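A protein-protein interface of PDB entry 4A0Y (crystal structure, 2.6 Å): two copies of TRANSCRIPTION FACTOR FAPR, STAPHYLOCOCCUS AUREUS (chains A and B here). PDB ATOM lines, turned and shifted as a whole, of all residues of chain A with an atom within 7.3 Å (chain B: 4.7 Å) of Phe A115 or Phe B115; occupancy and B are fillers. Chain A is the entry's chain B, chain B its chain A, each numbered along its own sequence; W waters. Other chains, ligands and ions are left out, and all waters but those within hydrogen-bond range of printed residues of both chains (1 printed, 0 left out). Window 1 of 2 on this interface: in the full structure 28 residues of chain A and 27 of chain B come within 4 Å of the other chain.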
ATOM      1  N   ILE A  73      23.297  22.447   6.095  1.00  0.00           N
ATOM      2  CA  ILE A  73      24.016  22.067   4.837  1.00  0.00           C
ATOM      3  C   ILE A  73      23.115  21.654   3.627  1.00  0.00           C
ATOM      4  O   ILE A  73      23.333  22.111   2.472  1.00  0.00           O
ATOM      5  CB  ILE A  73      25.313  21.123   5.090  1.00  0.00           C
ATOM      6  CG1 ILE A  73      26.586  21.846   4.639  1.00  0.00           C
ATOM      7  CG2 ILE A  73      25.297  19.813   4.293  1.00  0.00           C
ATOM      8  CD1 ILE A  73      27.036  23.034   5.532  1.00  0.00           C
ATOM      9  N   ILE A  79      28.279  25.691  -1.474  1.00  0.00           N
ATOM     10  CA  ILE A  79      28.930  25.770  -0.169  1.00  0.00           C
ATOM     11  C   ILE A  79      30.392  26.267  -0.238  1.00  0.00           C
ATOM     12  O   ILE A  79      31.210  25.711  -0.969  1.00  0.00           O
ATOM     13  CB  ILE A  79      28.843  24.420   0.593  1.00  0.00           C
ATOM     14  CG1 ILE A  79      27.417  24.150   1.063  1.00  0.00           C
ATOM     15  CG2 ILE A  79      29.741  24.408   1.831  1.00  0.00           C
ATOM     16  CD1 ILE A  79      26.561  23.360   0.098  1.00  0.00           C
ATOM     17  N   ARG A 110      32.151  17.716  10.077  1.00  0.00           N
ATOM     18  CA  ARG A 110      31.285  16.649   9.656  1.00  0.00           C
ATOM     19  C   ARG A 110      31.579  16.319   8.202  1.00  0.00           C
ATOM     20  O   ARG A 110      31.640  17.216   7.337  1.00  0.00           O
ATOM     21  CB  ARG A 110      29.853  17.100   9.801  1.00  0.00           C
ATOM     22  CG  ARG A 110      29.439  17.312  11.229  1.00  0.00           C
ATOM     23  CD  ARG A 110      28.791  16.031  11.785  1.00  0.00           C
ATOM     24  NE  ARG A 110      29.604  15.333  12.777  1.00  0.00           N
ATOM     25  CZ  ARG A 110      29.284  15.240  14.056  1.00  0.00           C
ATOM     26  NH1 ARG A 110      28.168  15.783  14.513  1.00  0.00           N
ATOM     27  NH2 ARG A 110      30.077  14.576  14.872  1.00  0.00           N
ATOM     28  N   GLY A 111      31.718  15.021   7.939  1.00  0.00           N
ATOM     29  CA  GLY A 111      32.028  14.504   6.610  1.00  0.00           C
ATOM     30  C   GLY A 111      31.223  15.196   5.550  1.00  0.00           C
ATOM     31  O   GLY A 111      31.772  15.597   4.518  1.00  0.00           O
ATOM     32  N   HIS A 112      29.923  15.369   5.828  1.00  0.00           N
ATOM     33  CA  HIS A 112      29.025  15.882   4.827  1.00  0.00           C
ATOM     34  C   HIS A 112      29.209  17.356   4.543  1.00  0.00           C
ATOM     35  O   HIS A 112      28.799  17.833   3.500  1.00  0.00           O
ATOM     36  CB  HIS A 112      27.552  15.541   5.114  1.00  0.00           C
ATOM     37  CG  HIS A 112      27.111  15.839   6.519  1.00  0.00           C
ATOM     38  ND1 HIS A 112      27.257  14.934   7.557  1.00  0.00           N
ATOM     39  CD2 HIS A 112      26.512  16.933   7.052  1.00  0.00           C
ATOM     40  CE1 HIS A 112      26.773  15.464   8.670  1.00  0.00           C
ATOM     41  NE2 HIS A 112      26.319  16.675   8.391  1.00  0.00           N
ATOM     42  N   VAL A 113      29.815  18.100   5.445  1.00  0.00           N
ATOM     43  CA  VAL A 113      30.126  19.475   5.107  1.00  0.00           C
ATOM     44  C   VAL A 113      31.200  19.489   4.007  1.00  0.00           C
ATOM     45  O   VAL A 113      31.035  20.148   2.973  1.00  0.00           O
ATOM     46  CB  VAL A 113      30.534  20.270   6.355  1.00  0.00           C
ATOM     47  CG1 VAL A 113      31.098  21.649   5.994  1.00  0.00           C
ATOM     48  CG2 VAL A 113      29.345  20.395   7.296  1.00  0.00           C
ATOM     49  N   LEU A 114      32.273  18.718   4.206  1.00  0.00           N
ATOM     50  CA  LEU A 114      33.341  18.650   3.206  1.00  0.00           C
ATOM     51  C   LEU A 114      32.814  18.091   1.902  1.00  0.00           C
ATOM     52  O   LEU A 114      33.204  18.565   0.838  1.00  0.00           O
ATOM     53  CB  LEU A 114      34.536  17.830   3.696  1.00  0.00           C
ATOM     54  CG  LEU A 114      35.094  18.164   5.082  1.00  0.00           C
ATOM     55  CD1 LEU A 114      36.323  17.338   5.336  1.00  0.00           C
ATOM     56  CD2 LEU A 114      35.440  19.627   5.209  1.00  0.00           C
ATOM     57  N   PHE A 115      31.929  17.096   1.976  1.00  0.00           N
ATOM     58  CA  PHE A 115      31.314  16.546   0.757  1.00  0.00           C
ATOM     59  C   PHE A 115      30.497  17.590  -0.003  1.00  0.00           C
ATOM     60  O   PHE A 115      30.628  17.710  -1.227  1.00  0.00           O
ATOM     61  CB  PHE A 115      30.439  15.326   1.030  1.00  0.00           C
ATOM     62  CG  PHE A 115      29.900  14.694  -0.220  1.00  0.00           C
ATOM     63  CD1 PHE A 115      30.643  13.744  -0.910  1.00  0.00           C
ATOM     64  CD2 PHE A 115      28.664  15.061  -0.727  1.00  0.00           C
ATOM     65  CE1 PHE A 115      30.151  13.173  -2.095  1.00  0.00           C
ATOM     66  CE2 PHE A 115      28.155  14.476  -1.881  1.00  0.00           C
ATOM     67  CZ  PHE A 115      28.910  13.535  -2.574  1.00  0.00           C
ATOM     68  N   ALA A 116      29.687  18.356   0.716  1.00  0.00           N
ATOM     69  CA  ALA A 116      28.907  19.390   0.082  1.00  0.00           C
ATOM     70  C   ALA A 116      29.800  20.430  -0.580  1.00  0.00           C
ATOM     71  O   ALA A 116      29.489  20.895  -1.674  1.00  0.00           O
ATOM     72  CB  ALA A 116      28.009  20.048   1.069  1.00  0.00           C
ATOM     73  N   GLN A 117      30.898  20.807   0.066  1.00  0.00           N
ATOM     74  CA  GLN A 117      31.820  21.729  -0.573  1.00  0.00           C
ATOM     75  C   GLN A 117      32.338  21.108  -1.864  1.00  0.00           C
ATOM     76  O   GLN A 117      32.328  21.761  -2.898  1.00  0.00           O
ATOM     77  CB  GLN A 117      32.988  22.096   0.331  1.00  0.00           C
ATOM     78  CG  GLN A 117      34.049  22.918  -0.355  1.00  0.00           C
ATOM     79  CD  GLN A 117      35.231  23.236   0.552  1.00  0.00           C
ATOM     80  OE1 GLN A 117      35.564  22.462   1.448  1.00  0.00           O
ATOM     81  NE2 GLN A 117      35.885  24.376   0.307  1.00  0.00           N
ATOM     82  N   ALA A 118      32.776  19.855  -1.826  1.00  0.00           N
ATOM     83  CA  ALA A 118      33.370  19.276  -3.021  1.00  0.00           C
ATOM     84  C   ALA A 118      32.340  19.144  -4.155  1.00  0.00           C
ATOM     85  O   ALA A 118      32.627  19.486  -5.301  1.00  0.00           O
ATOM     86  CB  ALA A 118      34.003  17.955  -2.710  1.00  0.00           C
ATOM     87  N   ASN A 119      31.148  18.660  -3.815  1.00  0.00           N
ATOM     88  CA  ASN A 119      30.140  18.334  -4.800  1.00  0.00           C
ATOM     89  C   ASN A 119      29.476  19.594  -5.310  1.00  0.00           C
ATOM     90  O   ASN A 119      29.096  19.676  -6.478  1.00  0.00           O
ATOM     91  CB  ASN A 119      29.078  17.411  -4.189  1.00  0.00           C
ATOM     92  CG  ASN A 119      27.948  17.039  -5.167  1.00  0.00           C
ATOM     93  OD1 ASN A 119      26.905  17.653  -5.140  1.00  0.00           O
ATOM     94  ND2 ASN A 119      28.146  16.024  -5.991  1.00  0.00           N
ATOM     95  N   SER A 120      29.327  20.598  -4.462  1.00  0.00           N
ATOM     96  CA  SER A 120      28.732  21.803  -4.981  1.00  0.00           C
ATOM     97  C   SER A 120      29.723  22.555  -5.889  1.00  0.00           C
ATOM     98  O   SER A 120      29.303  23.284  -6.806  1.00  0.00           O
ATOM     99  CB  SER A 120      28.074  22.657  -3.878  1.00  0.00           C
ATOM    100  OG  SER A 120      28.989  23.316  -3.034  1.00  0.00           O
ATOM    101  N   LEU A 121      31.024  22.319  -5.683  1.00  0.00           N
ATOM    102  CA  LEU A 121      32.080  22.886  -6.523  1.00  0.00           C
ATOM    103  C   LEU A 121      32.068  22.264  -7.910  1.00  0.00           C
ATOM    104  O   LEU A 121      32.269  22.986  -8.911  1.00  0.00           O
ATOM    105  CB  LEU A 121      33.451  22.739  -5.871  1.00  0.00           C
ATOM    106  CG  LEU A 121      34.632  23.413  -6.573  1.00  0.00           C
ATOM    107  CD1 LEU A 121      34.413  24.893  -6.753  1.00  0.00           C
ATOM    108  CD2 LEU A 121      35.928  23.208  -5.797  1.00  0.00           C
ATOM    109  N   THR A 133      24.696  14.631  -9.926  1.00  0.00           N
ATOM    110  CA  THR A 133      25.673  13.653  -9.457  1.00  0.00           C
ATOM    111  C   THR A 133      25.124  12.238  -9.647  1.00  0.00           C
ATOM    112  O   THR A 133      24.039  11.956  -9.138  1.00  0.00           O
ATOM    113  CB  THR A 133      25.918  13.871  -7.955  1.00  0.00           C
ATOM    114  OG1 THR A 133      26.105  15.272  -7.680  1.00  0.00           O
ATOM    115  CG2 THR A 133      27.104  13.065  -7.466  1.00  0.00           C
ATOM    116  N   GLU A 135      27.450   9.206  -9.279  1.00  0.00           N
ATOM    117  CA  GLU A 135      28.268   8.353  -8.388  1.00  0.00           C
ATOM    118  C   GLU A 135      29.416   9.120  -7.783  1.00  0.00           C
ATOM    119  O   GLU A 135      29.876  10.098  -8.336  1.00  0.00           O
ATOM    120  CB  GLU A 135      28.932   7.227  -9.162  1.00  0.00           C
ATOM    121  CG  GLU A 135      28.095   6.028  -9.412  1.00  0.00           C
ATOM    122  CD  GLU A 135      28.807   4.987 -10.303  1.00  0.00           C
ATOM    123  OE1 GLU A 135      30.019   4.725 -10.098  1.00  0.00           O
ATOM    124  OE2 GLU A 135      28.148   4.435 -11.225  1.00  0.00           O
ATOM    125  N   SER A 136      29.936   8.633  -6.674  1.00  0.00           N
ATOM    126  CA  SER A 136      31.053   9.297  -6.045  1.00  0.00           C
ATOM    127  C   SER A 136      31.768   8.378  -5.068  1.00  0.00           C
ATOM    128  O   SER A 136      31.135   7.570  -4.403  1.00  0.00           O
ATOM    129  CB  SER A 136      30.555  10.548  -5.324  1.00  0.00           C
ATOM    130  OG  SER A 136      31.652  11.248  -4.768  1.00  0.00           O
ATOM    131  N   SER A 137      33.082   8.509  -4.983  1.00  0.00           N
ATOM    132  CA  SER A 137      33.894   7.824  -3.959  1.00  0.00           C
ATOM    133  C   SER A 137      34.702   8.835  -3.214  1.00  0.00           C
ATOM    134  O   SER A 137      35.421   9.645  -3.834  1.00  0.00           O
ATOM    135  CB  SER A 137      34.886   6.919  -4.601  1.00  0.00           C
ATOM    136  OG  SER A 137      34.206   5.793  -5.000  1.00  0.00           O
ATOM    137  N   ILE A 138      34.619   8.809  -1.893  1.00  0.00           N
ATOM    138  CA  ILE A 138      35.289   9.841  -1.121  1.00  0.00           C
ATOM    139  C   ILE A 138      36.133   9.263   0.023  1.00  0.00           C
ATOM    140  O   ILE A 138      35.845   8.178   0.531  1.00  0.00           O
ATOM    141  CB  ILE A 138      34.274  10.871  -0.645  1.00  0.00           C
ATOM    142  CG1 ILE A 138      33.219  10.162   0.165  1.00  0.00           C
ATOM    143  CG2 ILE A 138      33.563  11.487  -1.856  1.00  0.00           C
ATOM    144  CD1 ILE A 138      32.155  11.072   0.662  1.00  0.00           C
ATOM    145  N   PHE A 140      37.941  10.664   3.653  1.00  0.00           N
ATOM    146  CA  PHE A 140      38.193  11.706   4.632  1.00  0.00           C
ATOM    147  C   PHE A 140      39.517  11.417   5.266  1.00  0.00           C
ATOM    148  O   PHE A 140      39.620  10.653   6.220  1.00  0.00           O
ATOM    149  CB  PHE A 140      37.039  11.747   5.640  1.00  0.00           C
ATOM    150  CG  PHE A 140      35.711  11.949   4.976  1.00  0.00           C
ATOM    151  CD1 PHE A 140      35.306  13.220   4.576  1.00  0.00           C
ATOM    152  CD2 PHE A 140      34.924  10.875   4.638  1.00  0.00           C
ATOM    153  CE1 PHE A 140      34.115  13.403   3.914  1.00  0.00           C
ATOM    154  CE2 PHE A 140      33.704  11.075   3.963  1.00  0.00           C
ATOM    155  CZ  PHE A 140      33.308  12.335   3.616  1.00  0.00           C
ATOM    156  N   SER A 170      40.823  18.295  -1.365  1.00  0.00           N
ATOM    157  CA  SER A 170      40.661  19.462  -0.492  1.00  0.00           C
ATOM    158  C   SER A 170      41.754  19.524   0.530  1.00  0.00           C
ATOM    159  O   SER A 170      42.149  18.502   1.076  1.00  0.00           O
ATOM    160  CB  SER A 170      39.341  19.437   0.233  1.00  0.00           C
ATOM    161  OG  SER A 170      38.268  19.299  -0.662  1.00  0.00           O
ATOM    162  N   PHE A 178      40.956  15.591   2.147  1.00  0.00           N
ATOM    163  CA  PHE A 178      39.771  15.013   1.504  1.00  0.00           C
ATOM    164  C   PHE A 178      40.015  14.779   0.041  1.00  0.00           C
ATOM    165  O   PHE A 178      40.544  15.639  -0.647  1.00  0.00           O
ATOM    166  CB  PHE A 178      38.582  15.974   1.639  1.00  0.00           C
ATOM    167  CG  PHE A 178      37.361  15.553   0.852  1.00  0.00           C
ATOM    168  CD1 PHE A 178      37.219  15.902  -0.493  1.00  0.00           C
ATOM    169  CD2 PHE A 178      36.326  14.837   1.463  1.00  0.00           C
ATOM    170  CE1 PHE A 178      36.105  15.503  -1.232  1.00  0.00           C
ATOM    171  CE2 PHE A 178      35.191  14.448   0.746  1.00  0.00           C
ATOM    172  CZ  PHE A 178      35.081  14.769  -0.600  1.00  0.00           C
ATOM    173  N   GLY A 180      37.801  13.251  -3.439  1.00  0.00           N
ATOM    174  CA  GLY A 180      36.597  12.656  -4.007  1.00  0.00           C
ATOM    175  C   GLY A 180      36.685  12.449  -5.497  1.00  0.00           C
ATOM    176  O   GLY A 180      37.284  13.260  -6.205  1.00  0.00           O
ATOM    177  N   ASN A 181      36.105  11.365  -5.985  1.00  0.00           N
ATOM    178  CA  ASN A 181      35.865  11.254  -7.413  1.00  0.00           C
ATOM    179  C   ASN A 181      34.388  11.377  -7.688  1.00  0.00           C
ATOM    180  O   ASN A 181      33.591  10.759  -6.991  1.00  0.00           O
ATOM    181  CB  ASN A 181      36.425   9.947  -7.937  1.00  0.00           C
ATOM    182  CG  ASN A 181      37.927   9.888  -7.770  1.00  0.00           C
ATOM    183  OD1 ASN A 181      38.644  10.789  -8.212  1.00  0.00           O
ATOM    184  ND2 ASN A 181      38.410   8.864  -7.069  1.00  0.00           N
ATOM    185  N   PHE A 182      34.013  12.181  -8.671  1.00  0.00           N
ATOM    186  CA  PHE A 182      32.599  12.401  -8.968  1.00  0.00           C
ATOM    187  C   PHE A 182      32.320  12.067 -10.391  1.00  0.00           C
ATOM    188  O   PHE A 182      33.021  12.549 -11.290  1.00  0.00           O
ATOM    189  CB  PHE A 182      32.186  13.859  -8.709  1.00  0.00           C
ATOM    190  CG  PHE A 182      32.326  14.277  -7.284  1.00  0.00           C
ATOM    191  CD1 PHE A 182      33.579  14.600  -6.759  1.00  0.00           C
ATOM    192  CD2 PHE A 182      31.218  14.306  -6.450  1.00  0.00           C
ATOM    193  CE1 PHE A 182      33.721  14.954  -5.427  1.00  0.00           C
ATOM    194  CE2 PHE A 182      31.351  14.673  -5.099  1.00  0.00           C
ATOM    195  CZ  PHE A 182      32.603  15.002  -4.592  1.00  0.00           C
ATOM    196  N   GLY B 111      22.883  16.685  -5.075  1.00  0.00           N
ATOM    197  CA  GLY B 111      23.629  15.490  -4.610  1.00  0.00           C
ATOM    198  C   GLY B 111      23.986  15.430  -3.118  1.00  0.00           C
ATOM    199  O   GLY B 111      23.864  14.353  -2.432  1.00  0.00           O
ATOM    200  N   HIS B 112      24.394  16.579  -2.598  1.00  0.00           N
ATOM    201  CA  HIS B 112      24.836  16.574  -1.256  1.00  0.00           C
ATOM    202  C   HIS B 112      23.743  16.474  -0.211  1.00  0.00           C
ATOM    203  O   HIS B 112      24.027  16.206   0.943  1.00  0.00           O
ATOM    204  CB  HIS B 112      25.699  17.770  -1.018  1.00  0.00           C
ATOM    205  CG  HIS B 112      24.953  19.052  -1.046  1.00  0.00           C
ATOM    206  ND1 HIS B 112      24.957  19.888  -2.147  1.00  0.00           N
ATOM    207  CD2 HIS B 112      24.200  19.661  -0.096  1.00  0.00           C
ATOM    208  CE1 HIS B 112      24.235  20.958  -1.864  1.00  0.00           C
ATOM    209  NE2 HIS B 112      23.783  20.854  -0.623  1.00  0.00           N
ATOM    210  N   VAL B 113      22.492  16.703  -0.589  1.00  0.00           N
ATOM    211  CA  VAL B 113      21.372  16.564   0.348  1.00  0.00           C
ATOM    212  C   VAL B 113      21.244  15.120   0.853  1.00  0.00           C
ATOM    213  O   VAL B 113      21.248  14.855   2.050  1.00  0.00           O
ATOM    214  CB  VAL B 113      20.098  16.991  -0.331  1.00  0.00           C
ATOM    215  CG1 VAL B 113      18.867  16.797   0.608  1.00  0.00           C
ATOM    216  CG2 VAL B 113      20.260  18.451  -0.816  1.00  0.00           C
ATOM    217  N   LEU B 114      21.163  14.183  -0.078  1.00  0.00           N
ATOM    218  CA  LEU B 114      20.980  12.809   0.276  1.00  0.00           C
ATOM    219  C   LEU B 114      22.243  12.266   0.939  1.00  0.00           C
ATOM    220  O   LEU B 114      22.158  11.475   1.865  1.00  0.00           O
ATOM    221  CB  LEU B 114      20.618  12.009  -0.966  1.00  0.00           C
ATOM    222  CG  LEU B 114      19.201  12.307  -1.484  1.00  0.00           C
ATOM    223  CD1 LEU B 114      19.067  12.023  -2.980  1.00  0.00           C
ATOM    224  CD2 LEU B 114      18.325  11.405  -0.753  1.00  0.00           C
ATOM    225  N   PHE B 115      23.425  12.700   0.501  1.00  0.00           N
ATOM    226  CA  PHE B 115      24.588  12.288   1.213  1.00  0.00           C
ATOM    227  C   PHE B 115      24.563  12.790   2.652  1.00  0.00           C
ATOM    228  O   PHE B 115      24.920  12.040   3.575  1.00  0.00           O
ATOM    229  CB  PHE B 115      25.890  12.701   0.524  1.00  0.00           C
ATOM    230  CG  PHE B 115      27.095  12.191   1.235  1.00  0.00           C
ATOM    231  CD1 PHE B 115      27.489  10.855   1.070  1.00  0.00           C
ATOM    232  CD2 PHE B 115      27.761  12.993   2.137  1.00  0.00           C
ATOM    233  CE1 PHE B 115      28.584  10.346   1.753  1.00  0.00           C
ATOM    234  CE2 PHE B 115      28.849  12.519   2.837  1.00  0.00           C
ATOM    235  CZ  PHE B 115      29.276  11.189   2.650  1.00  0.00           C
ATOM    236  N   ALA B 116      24.133  14.033   2.850  1.00  0.00           N
ATOM    237  CA  ALA B 116      24.062  14.589   4.190  1.00  0.00           C
ATOM    238  C   ALA B 116      23.129  13.791   5.107  1.00  0.00           C
ATOM    239  O   ALA B 116      23.458  13.601   6.279  1.00  0.00           O
ATOM    240  CB  ALA B 116      23.674  16.057   4.169  1.00  0.00           C
ATOM    241  N   GLN B 117      21.981  13.333   4.586  1.00  0.00           N
ATOM    242  CA  GLN B 117      21.069  12.501   5.375  1.00  0.00           C
ATOM    243  C   GLN B 117      21.794  11.184   5.719  1.00  0.00           C
ATOM    244  O   GLN B 117      21.789  10.731   6.866  1.00  0.00           O
ATOM    245  CB  GLN B 117      19.775  12.218   4.608  1.00  0.00           C
ATOM    246  CG  GLN B 117      18.840  11.290   5.348  1.00  0.00           C
ATOM    247  CD  GLN B 117      17.586  10.914   4.540  1.00  0.00           C
ATOM    248  OE1 GLN B 117      17.593  10.979   3.310  1.00  0.00           O
ATOM    249  NE2 GLN B 117      16.501  10.531   5.238  1.00  0.00           N
ATOM    250  N   ALA B 118      22.416  10.578   4.721  1.00  0.00           N
ATOM    251  CA  ALA B 118      22.998   9.271   4.901  1.00  0.00           C
ATOM    252  C   ALA B 118      24.166   9.337   5.924  1.00  0.00           C
ATOM    253  O   ALA B 118      24.224   8.562   6.888  1.00  0.00           O
ATOM    254  CB  ALA B 118      23.431   8.726   3.565  1.00  0.00           C
ATOM    255  N   ASN B 119      25.060  10.308   5.745  1.00  0.00           N
ATOM    256  CA  ASN B 119      26.204  10.436   6.619  1.00  0.00           C
ATOM    257  C   ASN B 119      25.791  10.694   8.060  1.00  0.00           C
ATOM    258  O   ASN B 119      26.328  10.046   8.977  1.00  0.00           O
ATOM    259  CB  ASN B 119      27.159  11.506   6.135  1.00  0.00           C
ATOM    260  CG  ASN B 119      28.543  11.394   6.790  1.00  0.00           C
ATOM    261  OD1 ASN B 119      29.314  10.366   6.416  1.00  0.00           O
ATOM    262  ND2 ASN B 119      28.903  12.218   7.630  1.00  0.00           N
ATOM    263  N   SER B 136      33.559   6.581   1.964  1.00  0.00           N
ATOM    264  CA  SER B 136      32.225   6.317   1.547  1.00  0.00           C
ATOM    265  C   SER B 136      32.191   6.109   0.062  1.00  0.00           C
ATOM    266  O   SER B 136      32.948   6.703  -0.691  1.00  0.00           O
ATOM    267  CB  SER B 136      31.324   7.483   1.957  1.00  0.00           C
ATOM    268  OG  SER B 136      30.019   7.238   1.510  1.00  0.00           O
ATOM    269  N   ILE B 138      29.168   5.975  -2.984  1.00  0.00           N
ATOM    270  CA  ILE B 138      27.710   6.194  -3.092  1.00  0.00           C
ATOM    271  C   ILE B 138      27.218   6.174  -4.510  1.00  0.00           C
ATOM    272  O   ILE B 138      27.962   6.558  -5.404  1.00  0.00           O
ATOM    273  CB  ILE B 138      27.285   7.547  -2.445  1.00  0.00           C
ATOM    274  CG1 ILE B 138      27.916   8.723  -3.182  1.00  0.00           C
ATOM    275  CG2 ILE B 138      27.641   7.596  -0.964  1.00  0.00           C
ATOM    276  CD1 ILE B 138      27.614  10.051  -2.515  1.00  0.00           C
ATOM    277  N   PHE B 178      18.905   5.849  -3.613  1.00  0.00           N
ATOM    278  CA  PHE B 178      20.251   6.131  -3.219  1.00  0.00           C
ATOM    279  C   PHE B 178      20.812   4.952  -2.485  1.00  0.00           C
ATOM    280  O   PHE B 178      20.098   4.300  -1.719  1.00  0.00           O
ATOM    281  CB  PHE B 178      20.240   7.346  -2.323  1.00  0.00           C
ATOM    282  CG  PHE B 178      21.555   7.686  -1.744  1.00  0.00           C
ATOM    283  CD1 PHE B 178      22.428   8.514  -2.432  1.00  0.00           C
ATOM    284  CD2 PHE B 178      21.907   7.215  -0.468  1.00  0.00           C
ATOM    285  CE1 PHE B 178      23.679   8.846  -1.881  1.00  0.00           C
ATOM    286  CE2 PHE B 178      23.131   7.552   0.119  1.00  0.00           C
ATOM    287  CZ  PHE B 178      24.030   8.364  -0.598  1.00  0.00           C
ATOM    288  N   PHE B 182      29.633   2.938   3.882  1.00  0.00           N
ATOM    289  CA  PHE B 182      30.292   3.856   4.772  1.00  0.00           C
ATOM    290  C   PHE B 182      31.263   3.131   5.678  1.00  0.00           C
ATOM    291  O   PHE B 182      30.900   2.165   6.358  1.00  0.00           O
ATOM    292  CB  PHE B 182      29.252   4.592   5.609  1.00  0.00           C
ATOM    293  CG  PHE B 182      28.463   5.617   4.824  1.00  0.00           C
ATOM    294  CD1 PHE B 182      27.412   5.219   3.984  1.00  0.00           C
ATOM    295  CD2 PHE B 182      28.778   6.968   4.911  1.00  0.00           C
ATOM    296  CE1 PHE B 182      26.699   6.162   3.242  1.00  0.00           C
ATOM    297  CE2 PHE B 182      28.051   7.941   4.181  1.00  0.00           C
ATOM    298  CZ  PHE B 182      27.019   7.529   3.338  1.00  0.00           C
HETATM  299  O   HOH W   1      23.881  17.196  -8.018  1.00  0.00           O
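The backbone NH (N) of Ile B138 sits at hydrogen-bond distance from the backbone carbonyl oxygen (O) of Ser A136, 2.9 Å away. The backbone NH (N) of Ile A138 is in hydrogen-bond range of the backbone carbonyl oxygen (O) of Ser B136. ND2 of Asn B119 is in hydrogen-bond range of ND1 of His A112, at 3.2 Å. A ring nitrogen (NE2) of His B112 is in hydrogen-bond range of the backbone carbonyl oxygen (O) of Ile A73.
The backbone NH (N) of Ile A79 sits at hydrogen-bond distance from the side-chain hydroxyl (OG) of Ser A120 (2.9 Å). OG of Ser A120 lies within hydrogen-bond range of O of Ala A116 (2.8 Å). The side-chain hydroxyl (OG) of Ser A136 sits at hydrogen-bond distance from the backbone carbonyl oxygen (O) of Asn A181, at 3.0 Å. The backbone NH of Asn A181 sits at hydrogen-bond distance from the backbone carbonyl oxygen of Ser A137 (2.8 Å). ND2 of Asn A119 sits at hydrogen-bond distance from OG1 of Thr A133 (2.8 Å).
Ile A79 touches His B112. His A112 touches Phe B115. His A112 touches Ala B116. CA of His B112 touches CE2 of Phe A115 (3.98 Å). CG of Phe A115 touches CD2 of Phe B115, at 3.6 Å. Phe A115 touches Ile B138. CA of Gly B111 touches OD1 of Asn A119, 3.96 Å away. His B112 touches Asn A119. CA of Ser A137 touches O of Ser B136, at 3.6 Å. Ile A138 touches Phe B115.
Phe B115 touches just these residues of chain A: His A112, Phe A115 and Ile A138. Of the printed residues of chain A, Gly B111 touches Asn A119 (3.96 Å) and Thr A133 (3.95 Å). Of the printed residues of chain B, Ser A137 touches Ser B136. Printed residues of chain A within 4 Å of Asn B119: Gly A111 and His A112. Of the printed residues of chain B, Thr A133 touches Gly B111 (3.95 Å). Of the printed residues of chain A, Ser B136 touches Ser A137 and Ile A138. Phe B178 touches none of the printed residues of chain A. Phe A182 touches none of the printed residues of chain B. The nearest residue of chain A that does not touch Phe B115 is Phe A140 (4.3 Å).
Hydrophobic or aromatic side chains of chain A within 4 Å of the printed part of chain B: Ile A79, His A112, Phe A115, Ala A116 and Ile A138. Among the printed residues, no Asp or Glu carboxylate lies within 4 Å of a Lys or Arg side-chain nitrogen of the other chain.
His A112 touches Ala B116, and with the chains exchanged Ala A116 touches His B112. His A112 touches Asn B119, and with the chains exchanged Asn A119 touches His B112. Phe B115 touches its own counterpart, Phe A115. Phe A115 touches Ile B138, and with the chains exchanged Ile A138 touches Phe B115. Positions printed for both chains: 111, 112, 113, 114, 115, 116, 117, 118, 119, 136, 138, 178 and 182.
Water W1 bridges the side-chain hydroxyl of Thr A133 (3.0 Å) and the backbone NH of Gly B111 (3.1 Å).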
